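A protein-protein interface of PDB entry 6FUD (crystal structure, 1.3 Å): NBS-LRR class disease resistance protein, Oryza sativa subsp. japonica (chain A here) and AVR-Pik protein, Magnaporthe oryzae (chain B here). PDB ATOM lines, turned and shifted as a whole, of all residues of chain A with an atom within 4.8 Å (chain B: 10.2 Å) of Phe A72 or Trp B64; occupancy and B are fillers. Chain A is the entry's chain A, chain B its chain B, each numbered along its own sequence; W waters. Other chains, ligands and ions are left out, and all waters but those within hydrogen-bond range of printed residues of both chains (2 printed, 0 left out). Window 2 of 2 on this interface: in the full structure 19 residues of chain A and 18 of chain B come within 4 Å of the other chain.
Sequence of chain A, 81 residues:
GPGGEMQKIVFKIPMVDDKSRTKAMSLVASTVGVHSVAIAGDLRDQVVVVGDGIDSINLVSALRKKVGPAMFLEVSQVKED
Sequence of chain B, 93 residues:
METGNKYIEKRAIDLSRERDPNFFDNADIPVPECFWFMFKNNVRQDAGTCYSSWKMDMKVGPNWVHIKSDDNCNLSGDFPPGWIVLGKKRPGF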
ATOM      1  N   ILE A   9      27.900  -5.156  22.072  1.00  0.00           N
ATOM      2  CA  ILE A   9      27.085  -6.346  22.198  1.00  0.00           C
ATOM      3  C   ILE A   9      27.604  -7.306  21.124  1.00  0.00           C
ATOM      4  O   ILE A   9      27.713  -6.932  19.951  1.00  0.00           O
ATOM      5  CB  ILE A   9      25.597  -6.053  21.934  1.00  0.00           C
ATOM      6  CG1 ILE A   9      25.014  -5.103  23.018  1.00  0.00           C
ATOM      7  CG2 ILE A   9      24.809  -7.361  21.879  1.00  0.00           C
ATOM      8  CD1 ILE A   9      23.869  -4.225  22.509  1.00  0.00           C
ATOM      9  N   VAL A  10      27.931  -8.535  21.496  1.00  0.00           N
ATOM     10  CA  VAL A  10      28.363  -9.511  20.486  1.00  0.00           C
ATOM     11  C   VAL A  10      27.406 -10.688  20.544  1.00  0.00           C
ATOM     12  O   VAL A  10      27.147 -11.255  21.617  1.00  0.00           O
ATOM     13  CB  VAL A  10      29.783 -10.003  20.767  1.00  0.00           C
ATOM     14  CG1 VAL A  10      30.227 -10.898  19.609  1.00  0.00           C
ATOM     15  CG2 VAL A  10      30.736  -8.816  20.951  1.00  0.00           C
ATOM     16  N   PHE A  11      26.847 -10.998  19.377  1.00  0.00           N
ATOM     17  CA  PHE A  11      26.008 -12.182  19.200  1.00  0.00           C
ATOM     18  C   PHE A  11      26.823 -13.266  18.491  1.00  0.00           C
ATOM     19  O   PHE A  11      27.751 -12.969  17.716  1.00  0.00           O
ATOM     20  CB  PHE A  11      24.814 -11.854  18.334  1.00  0.00           C
ATOM     21  CG  PHE A  11      23.892 -10.818  18.892  1.00  0.00           C
ATOM     22  CD1 PHE A  11      23.102 -11.122  19.973  1.00  0.00           C
ATOM     23  CD2 PHE A  11      23.836  -9.531  18.364  1.00  0.00           C
ATOM     24  CE1 PHE A  11      22.222 -10.199  20.501  1.00  0.00           C
ATOM     25  CE2 PHE A  11      22.972  -8.590  18.905  1.00  0.00           C
ATOM     26  CZ  PHE A  11      22.177  -8.925  19.968  1.00  0.00           C
ATOM     27  N   SER A  56      18.784  -4.317  23.076  1.00  0.00           N
ATOM     28  CA  SER A  56      19.419  -5.595  22.654  1.00  0.00           C
ATOM     29  C   SER A  56      18.477  -6.792  22.652  1.00  0.00           C
ATOM     30  O   SER A  56      18.674  -7.707  21.878  1.00  0.00           O
ATOM     31  CB  SER A  56      20.671  -5.926  23.482  1.00  0.00           C
ATOM     32  OG  SER A  56      20.327  -6.325  24.789  1.00  0.00           O
ATOM     33  N   ILE A  57      17.448  -6.774  23.497  1.00  0.00           N
ATOM     34  CA  ILE A  57      16.491  -7.889  23.544  1.00  0.00           C
ATOM     35  C   ILE A  57      15.614  -7.846  22.298  1.00  0.00           C
ATOM     36  O   ILE A  57      15.414  -8.870  21.631  1.00  0.00           O
ATOM     37  CB  ILE A  57      15.665  -7.899  24.864  1.00  0.00           C
ATOM     38  CG1 ILE A  57      16.595  -8.194  26.058  1.00  0.00           C
ATOM     39  CG2 ILE A  57      14.529  -8.919  24.796  1.00  0.00           C
ATOM     40  CD1 ILE A  57      17.010  -9.659  26.205  1.00  0.00           C
ATOM     41  N   VAL A  60      17.939  -9.138  19.407  1.00  0.00           N
ATOM     42  CA  VAL A  60      18.146 -10.588  19.306  1.00  0.00           C
ATOM     43  C   VAL A  60      16.885 -11.314  18.811  1.00  0.00           C
ATOM     44  O   VAL A  60      16.975 -12.271  18.054  1.00  0.00           O
ATOM     45  CB  VAL A  60      18.676 -11.207  20.617  1.00  0.00           C
ATOM     46  CG1 VAL A  60      17.564 -11.392  21.664  1.00  0.00           C
ATOM     47  CG2 VAL A  60      19.438 -12.478  20.285  1.00  0.00           C
ATOM     48  N   ALA A  70      20.165 -16.682  16.966  1.00  0.00           N
ATOM     49  CA  ALA A  70      21.150 -15.834  17.571  1.00  0.00           C
ATOM     50  C   ALA A  70      21.193 -16.011  19.077  1.00  0.00           C
ATOM     51  O   ALA A  70      20.175 -16.209  19.731  1.00  0.00           O
ATOM     52  CB  ALA A  70      20.857 -14.388  17.252  1.00  0.00           C
ATOM     53  N   MET A  71      22.402 -15.929  19.596  1.00  0.00           N
ATOM     54  CA  MET A  71      22.586 -15.965  21.027  1.00  0.00           C
ATOM     55  C   MET A  71      23.536 -14.886  21.445  1.00  0.00           C
ATOM     56  O   MET A  71      24.422 -14.509  20.707  1.00  0.00           O
ATOM     57  CB  MET A  71      23.195 -17.290  21.377  1.00  0.00           C
ATOM     58  CG  MET A  71      22.366 -18.389  20.735  1.00  0.00           C
ATOM     59  SD  MET A  71      22.549 -20.003  21.422  1.00  0.00           S
ATOM     60  CE  MET A  71      23.804 -20.501  20.338  1.00  0.00           C
ATOM     61  N   PHE A  72      23.333 -14.354  22.636  1.00  0.00           N
ATOM     62  CA  PHE A  72      24.307 -13.467  23.225  1.00  0.00           C
ATOM     63  C   PHE A  72      25.652 -14.180  23.497  1.00  0.00           C
ATOM     64  O   PHE A  72      25.700 -15.296  24.037  1.00  0.00           O
ATOM     65  CB  PHE A  72      23.742 -12.879  24.521  1.00  0.00           C
ATOM     66  CG  PHE A  72      22.711 -11.805  24.322  1.00  0.00           C
ATOM     67  CD1 PHE A  72      23.097 -10.479  24.200  1.00  0.00           C
ATOM     68  CD2 PHE A  72      21.341 -12.097  24.330  1.00  0.00           C
ATOM     69  CE1 PHE A  72      22.178  -9.464  24.097  1.00  0.00           C
ATOM     70  CE2 PHE A  72      20.427 -11.076  24.202  1.00  0.00           C
ATOM     71  CZ  PHE A  72      20.831  -9.763  24.072  1.00  0.00           C
ATOM     72  N   LEU A  73      26.741 -13.532  23.138  1.00  0.00           N
ATOM     73  CA  LEU A  73      28.090 -13.972  23.551  1.00  0.00           C
ATOM     74  C   LEU A  73      28.637 -12.956  24.585  1.00  0.00           C
ATOM     75  O   LEU A  73      29.237 -13.372  25.557  1.00  0.00           O
ATOM     76  CB  LEU A  73      29.008 -14.044  22.352  1.00  0.00           C
ATOM     77  CG  LEU A  73      30.448 -14.259  22.683  1.00  0.00           C
ATOM     78  CD1 LEU A  73      30.764 -15.573  23.412  1.00  0.00           C
ATOM     79  CD2 LEU A  73      31.296 -14.177  21.411  1.00  0.00           C
ATOM     80  N   GLU A  74      28.464 -11.655  24.352  1.00  0.00           N
ATOM     81  CA  GLU A  74      29.006 -10.660  25.274  1.00  0.00           C
ATOM     82  C   GLU A  74      28.129  -9.446  25.350  1.00  0.00           C
ATOM     83  O   GLU A  74      27.594  -8.995  24.350  1.00  0.00           O
ATOM     84  CB  GLU A  74      30.335 -10.222  24.725  1.00  0.00           C
ATOM     85  CG  GLU A  74      30.975  -9.070  25.435  1.00  0.00           C
ATOM     86  CD  GLU A  74      32.263  -8.642  24.801  1.00  0.00           C
ATOM     87  OE1 GLU A  74      32.823  -9.394  23.974  1.00  0.00           O
ATOM     88  OE2 GLU A  74      32.740  -7.510  25.106  1.00  0.00           O
ATOM     89  N   VAL A  75      28.058  -8.866  26.559  1.00  0.00           N
ATOM     90  CA  VAL A  75      27.526  -7.512  26.740  1.00  0.00           C
ATOM     91  C   VAL A  75      28.558  -6.744  27.555  1.00  0.00           C
ATOM     92  O   VAL A  75      28.957  -7.219  28.614  1.00  0.00           O
ATOM     93  CB  VAL A  75      26.184  -7.544  27.468  1.00  0.00           C
ATOM     94  CG1 VAL A  75      25.718  -6.153  27.733  1.00  0.00           C
ATOM     95  CG2 VAL A  75      25.164  -8.315  26.638  1.00  0.00           C
ATOM     96  N   TRP B  36      41.319 -12.449  23.422  1.00  0.00           N
ATOM     97  CA  TRP B  36      40.808 -13.504  24.291  1.00  0.00           C
ATOM     98  C   TRP B  36      40.550 -14.776  23.477  1.00  0.00           C
ATOM     99  O   TRP B  36      40.215 -14.696  22.284  1.00  0.00           O
ATOM    100  CB  TRP B  36      39.494 -13.118  25.018  1.00  0.00           C
ATOM    101  CG  TRP B  36      38.314 -12.762  24.166  1.00  0.00           C
ATOM    102  CD1 TRP B  36      37.894 -11.508  23.834  1.00  0.00           C
ATOM    103  CD2 TRP B  36      37.350 -13.657  23.585  1.00  0.00           C
ATOM    104  NE1 TRP B  36      36.777 -11.565  23.057  1.00  0.00           N
ATOM    105  CE2 TRP B  36      36.430 -12.884  22.885  1.00  0.00           C
ATOM    106  CE3 TRP B  36      37.207 -15.033  23.563  1.00  0.00           C
ATOM    107  CZ2 TRP B  36      35.366 -13.456  22.177  1.00  0.00           C
ATOM    108  CZ3 TRP B  36      36.162 -15.593  22.843  1.00  0.00           C
ATOM    109  CH2 TRP B  36      35.288 -14.826  22.159  1.00  0.00           C
ATOM    110  N   MET B  38      38.600 -18.626  24.046  1.00  0.00           N
ATOM    111  CA  MET B  38      37.722 -19.453  24.876  1.00  0.00           C
ATOM    112  C   MET B  38      37.964 -20.923  24.582  1.00  0.00           C
ATOM    113  O   MET B  38      37.932 -21.307  23.406  1.00  0.00           O
ATOM    114  CB  MET B  38      36.276 -19.082  24.623  1.00  0.00           C
ATOM    115  CG  MET B  38      35.277 -19.855  25.454  1.00  0.00           C
ATOM    116  SD  MET B  38      33.543 -19.512  25.123  1.00  0.00           S
ATOM    117  CE  MET B  38      33.487 -17.784  25.379  1.00  0.00           C
ATOM    118  N   ASP B  46      36.144 -20.205  20.346  1.00  0.00           N
ATOM    119  CA  ASP B  46      36.165 -18.960  19.573  1.00  0.00           C
ATOM    120  C   ASP B  46      37.199 -18.060  20.227  1.00  0.00           C
ATOM    121  O   ASP B  46      37.821 -18.438  21.261  1.00  0.00           O
ATOM    122  CB  ASP B  46      34.787 -18.327  19.419  1.00  0.00           C
ATOM    123  CG  ASP B  46      34.618 -17.536  18.117  1.00  0.00           C
ATOM    124  OD1 ASP B  46      35.641 -17.169  17.482  1.00  0.00           O
ATOM    125  OD2 ASP B  46      33.441 -17.227  17.794  1.00  0.00           O
ATOM    126  N   MET B  56      33.746  -7.323  31.327  1.00  0.00           N
ATOM    127  CA  MET B  56      32.729  -7.695  30.375  1.00  0.00           C
ATOM    128  C   MET B  56      31.929  -8.856  30.935  1.00  0.00           C
ATOM    129  O   MET B  56      32.462  -9.641  31.710  1.00  0.00           O
ATOM    130  CB  MET B  56      33.333  -8.064  29.006  1.00  0.00           C
ATOM    131  CG  MET B  56      34.321  -9.206  29.062  1.00  0.00           C
ATOM    132  SD  MET B  56      35.048  -9.482  27.374  1.00  0.00           S
ATOM    133  CE  MET B  56      36.234 -10.735  27.767  1.00  0.00           C
ATOM    134  N   ASP B  57      30.713  -8.997  30.473  1.00  0.00           N
ATOM    135  CA  ASP B  57      29.942 -10.222  30.742  1.00  0.00           C
ATOM    136  C   ASP B  57      29.954 -11.041  29.465  1.00  0.00           C
ATOM    137  O   ASP B  57      29.624 -10.534  28.397  1.00  0.00           O
ATOM    138  CB  ASP B  57      28.520  -9.838  31.138  1.00  0.00           C
ATOM    139  CG  ASP B  57      28.527  -9.139  32.497  1.00  0.00           C
ATOM    140  OD1 ASP B  57      29.109  -9.668  33.451  1.00  0.00           O
ATOM    141  OD2 ASP B  57      27.982  -8.012  32.598  1.00  0.00           O
ATOM    142  N   MET B  58      30.360 -12.310  29.637  1.00  0.00           N
ATOM    143  CA  MET B  58      30.494 -13.205  28.463  1.00  0.00           C
ATOM    144  C   MET B  58      29.835 -14.521  28.802  1.00  0.00           C
ATOM    145  O   MET B  58      29.967 -15.069  29.883  1.00  0.00           O
ATOM    146  CB  MET B  58      31.997 -13.408  28.153  1.00  0.00           C
ATOM    147  CG  MET B  58      32.251 -14.311  26.959  1.00  0.00           C
ATOM    148  SD  MET B  58      33.977 -14.351  26.449  1.00  0.00           S
ATOM    149  CE  MET B  58      34.046 -12.765  25.555  1.00  0.00           C
ATOM    150  N   LYS B  59      29.154 -15.073  27.789  1.00  0.00           N
ATOM    151  CA  LYS B  59      28.524 -16.395  27.941  1.00  0.00           C
ATOM    152  C   LYS B  59      29.568 -17.442  27.618  1.00  0.00           C
ATOM    153  O   LYS B  59      30.091 -17.474  26.487  1.00  0.00           O
ATOM    154  CB  LYS B  59      27.312 -16.495  27.005  1.00  0.00           C
ATOM    155  CG  LYS B  59      26.485 -17.767  27.269  1.00  0.00           C
ATOM    156  CD  LYS B  59      25.711 -17.712  28.611  1.00  0.00           C
ATOM    157  CE  LYS B  59      24.862 -18.908  28.878  1.00  0.00           C
ATOM    158  NZ  LYS B  59      23.724 -18.858  27.964  1.00  0.00           N
ATOM    159  N   VAL B  60      29.873 -18.256  28.592  1.00  0.00           N
ATOM    160  CA  VAL B  60      30.912 -19.282  28.484  1.00  0.00           C
ATOM    161  C   VAL B  60      30.206 -20.641  28.659  1.00  0.00           C
ATOM    162  O   VAL B  60      29.851 -21.034  29.752  1.00  0.00           O
ATOM    163  CB  VAL B  60      32.022 -19.089  29.531  1.00  0.00           C
ATOM    164  CG1 VAL B  60      33.076 -20.153  29.377  1.00  0.00           C
ATOM    165  CG2 VAL B  60      32.586 -17.662  29.458  1.00  0.00           C
ATOM    166  N   GLY B  61      29.904 -21.284  27.532  1.00  0.00           N
ATOM    167  CA  GLY B  61      29.106 -22.508  27.570  1.00  0.00           C
ATOM    168  C   GLY B  61      27.769 -22.242  28.210  1.00  0.00           C
ATOM    169  O   GLY B  61      27.053 -21.339  27.771  1.00  0.00           O
ATOM    170  N   PRO B  62      27.464 -22.954  29.323  1.00  0.00           N
ATOM    171  CA  PRO B  62      26.135 -22.856  29.929  1.00  0.00           C
ATOM    172  C   PRO B  62      25.999 -21.725  30.978  1.00  0.00           C
ATOM    173  O   PRO B  62      24.915 -21.585  31.570  1.00  0.00           O
ATOM    174  CB  PRO B  62      25.980 -24.173  30.647  1.00  0.00           C
ATOM    175  CG  PRO B  62      27.401 -24.522  31.077  1.00  0.00           C
ATOM    176  CD  PRO B  62      28.253 -24.040  29.925  1.00  0.00           C
ATOM    177  N   ASN B  63      27.052 -20.926  31.195  1.00  0.00           N
ATOM    178  CA  ASN B  63      27.008 -19.918  32.247  1.00  0.00           C
ATOM    179  C   ASN B  63      27.543 -18.570  31.768  1.00  0.00           C
ATOM    180  O   ASN B  63      28.615 -18.492  31.151  1.00  0.00           O
ATOM    181  CB  ASN B  63      27.821 -20.333  33.468  1.00  0.00           C
ATOM    182  CG  ASN B  63      27.319 -21.645  34.062  1.00  0.00           C
ATOM    183  OD1 ASN B  63      26.251 -21.710  34.705  1.00  0.00           O
ATOM    184  ND2 ASN B  63      28.007 -22.690  33.786  1.00  0.00           N
ATOM    185  N   TRP B  64      26.859 -17.487  32.174  1.00  0.00           N
ATOM    186  CA  TRP B  64      27.465 -16.170  32.111  1.00  0.00           C
ATOM    187  C   TRP B  64      28.617 -16.082  33.103  1.00  0.00           C
ATOM    188  O   TRP B  64      28.531 -16.598  34.246  1.00  0.00           O
ATOM    189  CB  TRP B  64      26.422 -15.092  32.458  1.00  0.00           C
ATOM    190  CG  TRP B  64      25.471 -14.858  31.322  1.00  0.00           C
ATOM    191  CD1 TRP B  64      24.240 -15.415  31.136  1.00  0.00           C
ATOM    192  CD2 TRP B  64      25.720 -14.049  30.177  1.00  0.00           C
ATOM    193  NE1 TRP B  64      23.708 -14.965  29.949  1.00  0.00           N
ATOM    194  CE2 TRP B  64      24.621 -14.156  29.320  1.00  0.00           C
ATOM    195  CE3 TRP B  64      26.783 -13.208  29.806  1.00  0.00           C
ATOM    196  CZ2 TRP B  64      24.528 -13.432  28.132  1.00  0.00           C
ATOM    197  CZ3 TRP B  64      26.740 -12.541  28.604  1.00  0.00           C
ATOM    198  CH2 TRP B  64      25.626 -12.663  27.763  1.00  0.00           C
ATOM    199  N   VAL B  65      29.648 -15.382  32.645  1.00  0.00           N
ATOM    200  CA  VAL B  65      30.834 -15.152  33.482  1.00  0.00           C
ATOM    201  C   VAL B  65      31.095 -13.642  33.421  1.00  0.00           C
ATOM    202  O   VAL B  65      31.133 -13.044  32.342  1.00  0.00           O
ATOM    203  CB  VAL B  65      32.056 -15.967  32.995  1.00  0.00           C
ATOM    204  CG1 VAL B  65      33.235 -15.777  33.915  1.00  0.00           C
ATOM    205  CG2 VAL B  65      31.700 -17.448  32.904  1.00  0.00           C
ATOM    206  N   HIS B  66      31.369 -13.052  34.581  1.00  0.00           N
ATOM    207  CA  HIS B  66      31.832 -11.673  34.652  1.00  0.00           C
ATOM    208  C   HIS B  66      33.356 -11.687  34.618  1.00  0.00           C
ATOM    209  O   HIS B  66      33.984 -12.194  35.550  1.00  0.00           O
ATOM    210  CB  HIS B  66      31.317 -11.020  35.918  1.00  0.00           C
ATOM    211  CG  HIS B  66      31.661  -9.572  35.974  1.00  0.00           C
ATOM    212  ND1 HIS B  66      31.037  -8.639  35.198  1.00  0.00           N
ATOM    213  CD2 HIS B  66      32.598  -8.879  36.706  1.00  0.00           C
ATOM    214  CE1 HIS B  66      31.561  -7.446  35.449  1.00  0.00           C
ATOM    215  NE2 HIS B  66      32.545  -7.583  36.299  1.00  0.00           N
ATOM    216  N   ILE B  67      33.939 -11.240  33.535  1.00  0.00           N
ATOM    217  CA  ILE B  67      35.360 -11.364  33.285  1.00  0.00           C
ATOM    218  C   ILE B  67      36.032 -10.011  33.461  1.00  0.00           C
ATOM    219  O   ILE B  67      35.637  -9.037  32.817  1.00  0.00           O
ATOM    220  CB  ILE B  67      35.652 -11.910  31.890  1.00  0.00           C
ATOM    221  CG1 ILE B  67      34.999 -13.298  31.688  1.00  0.00           C
ATOM    222  CG2 ILE B  67      37.145 -11.982  31.645  1.00  0.00           C
ATOM    223  CD1 ILE B  67      35.168 -13.893  30.301  1.00  0.00           C
ATOM    224  N   SER B  76      40.187 -12.771  34.640  1.00  0.00           N
ATOM    225  CA  SER B  76      39.703 -13.405  35.837  1.00  0.00           C
ATOM    226  C   SER B  76      38.189 -13.539  35.801  1.00  0.00           C
ATOM    227  O   SER B  76      37.504 -12.633  35.394  1.00  0.00           O
ATOM    228  CB  SER B  76      40.092 -12.543  37.112  1.00  0.00           C
ATOM    229  OG  SER B  76      41.448 -12.405  37.224  1.00  0.00           O
ATOM    230  N   GLY B  77      37.687 -14.673  36.238  1.00  0.00           N
ATOM    231  CA  GLY B  77      36.273 -14.877  36.329  1.00  0.00           C
ATOM    232  C   GLY B  77      35.942 -16.238  36.914  1.00  0.00           C
ATOM    233  O   GLY B  77      36.809 -17.066  37.081  1.00  0.00           O
ATOM    234  N   ASP B  78      34.679 -16.436  37.246  1.00  0.00           N
ATOM    235  CA  ASP B  78      34.164 -17.715  37.754  1.00  0.00           C
ATOM    236  C   ASP B  78      33.753 -18.592  36.584  1.00  0.00           C
ATOM    237  O   ASP B  78      32.579 -18.679  36.277  1.00  0.00           O
ATOM    238  CB  ASP B  78      32.992 -17.440  38.728  1.00  0.00           C
ATOM    239  CG  ASP B  78      32.490 -18.694  39.425  1.00  0.00           C
ATOM    240  OD1 ASP B  78      33.203 -19.707  39.415  1.00  0.00           O
ATOM    241  OD2 ASP B  78      31.406 -18.652  40.035  1.00  0.00           O
ATOM    242  N   PHE B  79      34.733 -19.216  35.943  1.00  0.00           N
ATOM    243  CA  PHE B  79      34.448 -20.041  34.769  1.00  0.00           C
ATOM    244  C   PHE B  79      33.891 -21.402  35.144  1.00  0.00           C
ATOM    245  O   PHE B  79      34.273 -21.975  36.135  1.00  0.00           O
ATOM    246  CB  PHE B  79      35.739 -20.262  33.974  1.00  0.00           C
ATOM    247  CG  PHE B  79      36.343 -18.997  33.468  1.00  0.00           C
ATOM    248  CD1 PHE B  79      35.777 -18.317  32.432  1.00  0.00           C
ATOM    249  CD2 PHE B  79      37.475 -18.454  34.067  1.00  0.00           C
ATOM    250  CE1 PHE B  79      36.305 -17.135  31.987  1.00  0.00           C
ATOM    251  CE2 PHE B  79      38.025 -17.290  33.563  1.00  0.00           C
ATOM    252  CZ  PHE B  79      37.419 -16.625  32.552  1.00  0.00           C
ATOM    253  N   PRO B  80      32.925 -21.913  34.359  1.00  0.00           N
ATOM    254  CA  PRO B  80      32.363 -23.230  34.656  1.00  0.00           C
ATOM    255  C   PRO B  80      33.395 -24.321  34.465  1.00  0.00           C
ATOM    256  O   PRO B  80      34.367 -24.137  33.748  1.00  0.00           O
ATOM    257  CB  PRO B  80      31.171 -23.356  33.684  1.00  0.00           C
ATOM    258  CG  PRO B  80      31.464 -22.423  32.581  1.00  0.00           C
ATOM    259  CD  PRO B  80      32.244 -21.281  33.210  1.00  0.00           C
ATOM    260  N   PRO B  81      33.183 -25.478  35.132  1.00  0.00           N
ATOM    261  CA  PRO B  81      34.184 -26.531  35.059  1.00  0.00           C
ATOM    262  C   PRO B  81      34.528 -26.945  33.635  1.00  0.00           C
ATOM    263  O   PRO B  81      33.651 -27.157  32.767  1.00  0.00           O
ATOM    264  CB  PRO B  81      33.521 -27.694  35.847  1.00  0.00           C
ATOM    265  CG  PRO B  81      32.605 -27.025  36.754  1.00  0.00           C
ATOM    266  CD  PRO B  81      32.067 -25.837  36.048  1.00  0.00           C
ATOM    267  N   TRP B  83      36.056 -25.056  31.488  1.00  0.00           N
ATOM    268  CA  TRP B  83      36.119 -23.921  30.556  1.00  0.00           C
ATOM    269  C   TRP B  83      37.094 -22.903  31.047  1.00  0.00           C
ATOM    270  O   TRP B  83      37.272 -22.706  32.266  1.00  0.00           O
ATOM    271  CB  TRP B  83      34.756 -23.226  30.516  1.00  0.00           C
ATOM    272  CG  TRP B  83      33.652 -24.039  29.832  1.00  0.00           C
ATOM    273  CD1 TRP B  83      32.831 -24.986  30.378  1.00  0.00           C
ATOM    274  CD2 TRP B  83      33.242 -23.878  28.478  1.00  0.00           C
ATOM    275  NE1 TRP B  83      31.960 -25.431  29.425  1.00  0.00           N
ATOM    276  CE2 TRP B  83      32.172 -24.767  28.256  1.00  0.00           C
ATOM    277  CE3 TRP B  83      33.660 -23.057  27.440  1.00  0.00           C
ATOM    278  CZ2 TRP B  83      31.531 -24.872  26.995  1.00  0.00           C
ATOM    279  CZ3 TRP B  83      33.013 -23.129  26.235  1.00  0.00           C
ATOM    280  CH2 TRP B  83      31.959 -24.032  26.020  1.00  0.00           C
ATOM    281  N   VAL B  85      38.565 -18.729  29.660  1.00  0.00           N
ATOM    282  CA  VAL B  85      38.854 -17.682  28.668  1.00  0.00           C
ATOM    283  C   VAL B  85      40.213 -17.103  29.058  1.00  0.00           C
ATOM    284  O   VAL B  85      40.372 -16.673  30.199  1.00  0.00           O
ATOM    285  CB  VAL B  85      37.748 -16.621  28.592  1.00  0.00           C
ATOM    286  CG1 VAL B  85      38.079 -15.605  27.519  1.00  0.00           C
ATOM    287  CG2 VAL B  85      36.361 -17.270  28.339  1.00  0.00           C
HETATM  288  O   HOH W   1      34.872  -9.362  22.458  1.00  0.00           O
HETATM  289  O   HOH W   2      27.448  -6.372  30.788  1.00  0.00           O
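N of Lys B59 lies within hydrogen-bond range of O of Leu A73, 2.8 Å away. The backbone NH of Val A75 is in hydrogen-bond range of the backbone carbonyl oxygen of Asp B57. The side-chain carboxylate (OE2) of Glu A74 lies close to the side-chain sulfur (SD) of Met B56 (3.8 Å).
N of Leu A73 lies within hydrogen-bond range of O of Val A10 (2.8 Å). N of Val B65 sits at hydrogen-bond distance from O of Met B58 (2.8 Å). O of Met B56 sits at hydrogen-bond distance from N of Ile B67 (2.8 Å). A ring nitrogen (ND1) of His B66 lies within hydrogen-bond range of the side-chain carboxylate of Asp B57, at 2.8 Å. N of Val A10 lies within hydrogen-bond range of O of Glu A74, at 2.9 Å.
Among the printed residues, pairs that only touch across the chains: Leu A73 with Met B58 (3.2 Å), Glu A74 with Asp B57 (3.2 Å), Phe A72 with Lys B59 (3.6 Å), Phe A72 with Trp B64 (3.7 Å) and Glu A74 with Met B58 (3.9 Å).
No residue of chain B comes within 4 Å of Ser A56. Phe A72 touches two residues of chain B. Of the printed residues of chain A, Met B56 touches Glu A74 (3.8 Å). Printed residues of chain A within 4 Å of Asp B57: Glu A74 and Val A75. Printed residues of chain A within 4 Å of Met B58: Leu A73 and Glu A74. Of the printed residues of chain A, Lys B59 touches Phe A72 and Leu A73. Of chain A, only Phe A72 comes within 4 Å of Trp B64. The nearest residue of chain A that does not touch Trp B64 is Leu A73 (4.03 Å). The nearest printed residue of chain A that does not touch Met B56 is Val A75 (4.1 Å).
Of the 23 printed residues of chain B, 5 touch a printed residue of chain A. Hydrophobic or aromatic side chains of chain B that line the printed part of chain A: Met B56, Met B58 and Trp B64. Of the 12 printed residues of chain A, 4 touch a printed residue of chain B. Among the printed residues, no Asp or Glu carboxylate lies within 4 Å of a Lys or Arg side-chain nitrogen of the other chain.
Water W2 bridges OD2 of Asp B57 (2.5 Å) and O of Val A75 (2.8 Å). Water W1 lies within hydrogen-bond range of OE1 of Glu A74 (2.5 Å) and NE1 of Trp B36 (3.0 Å).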
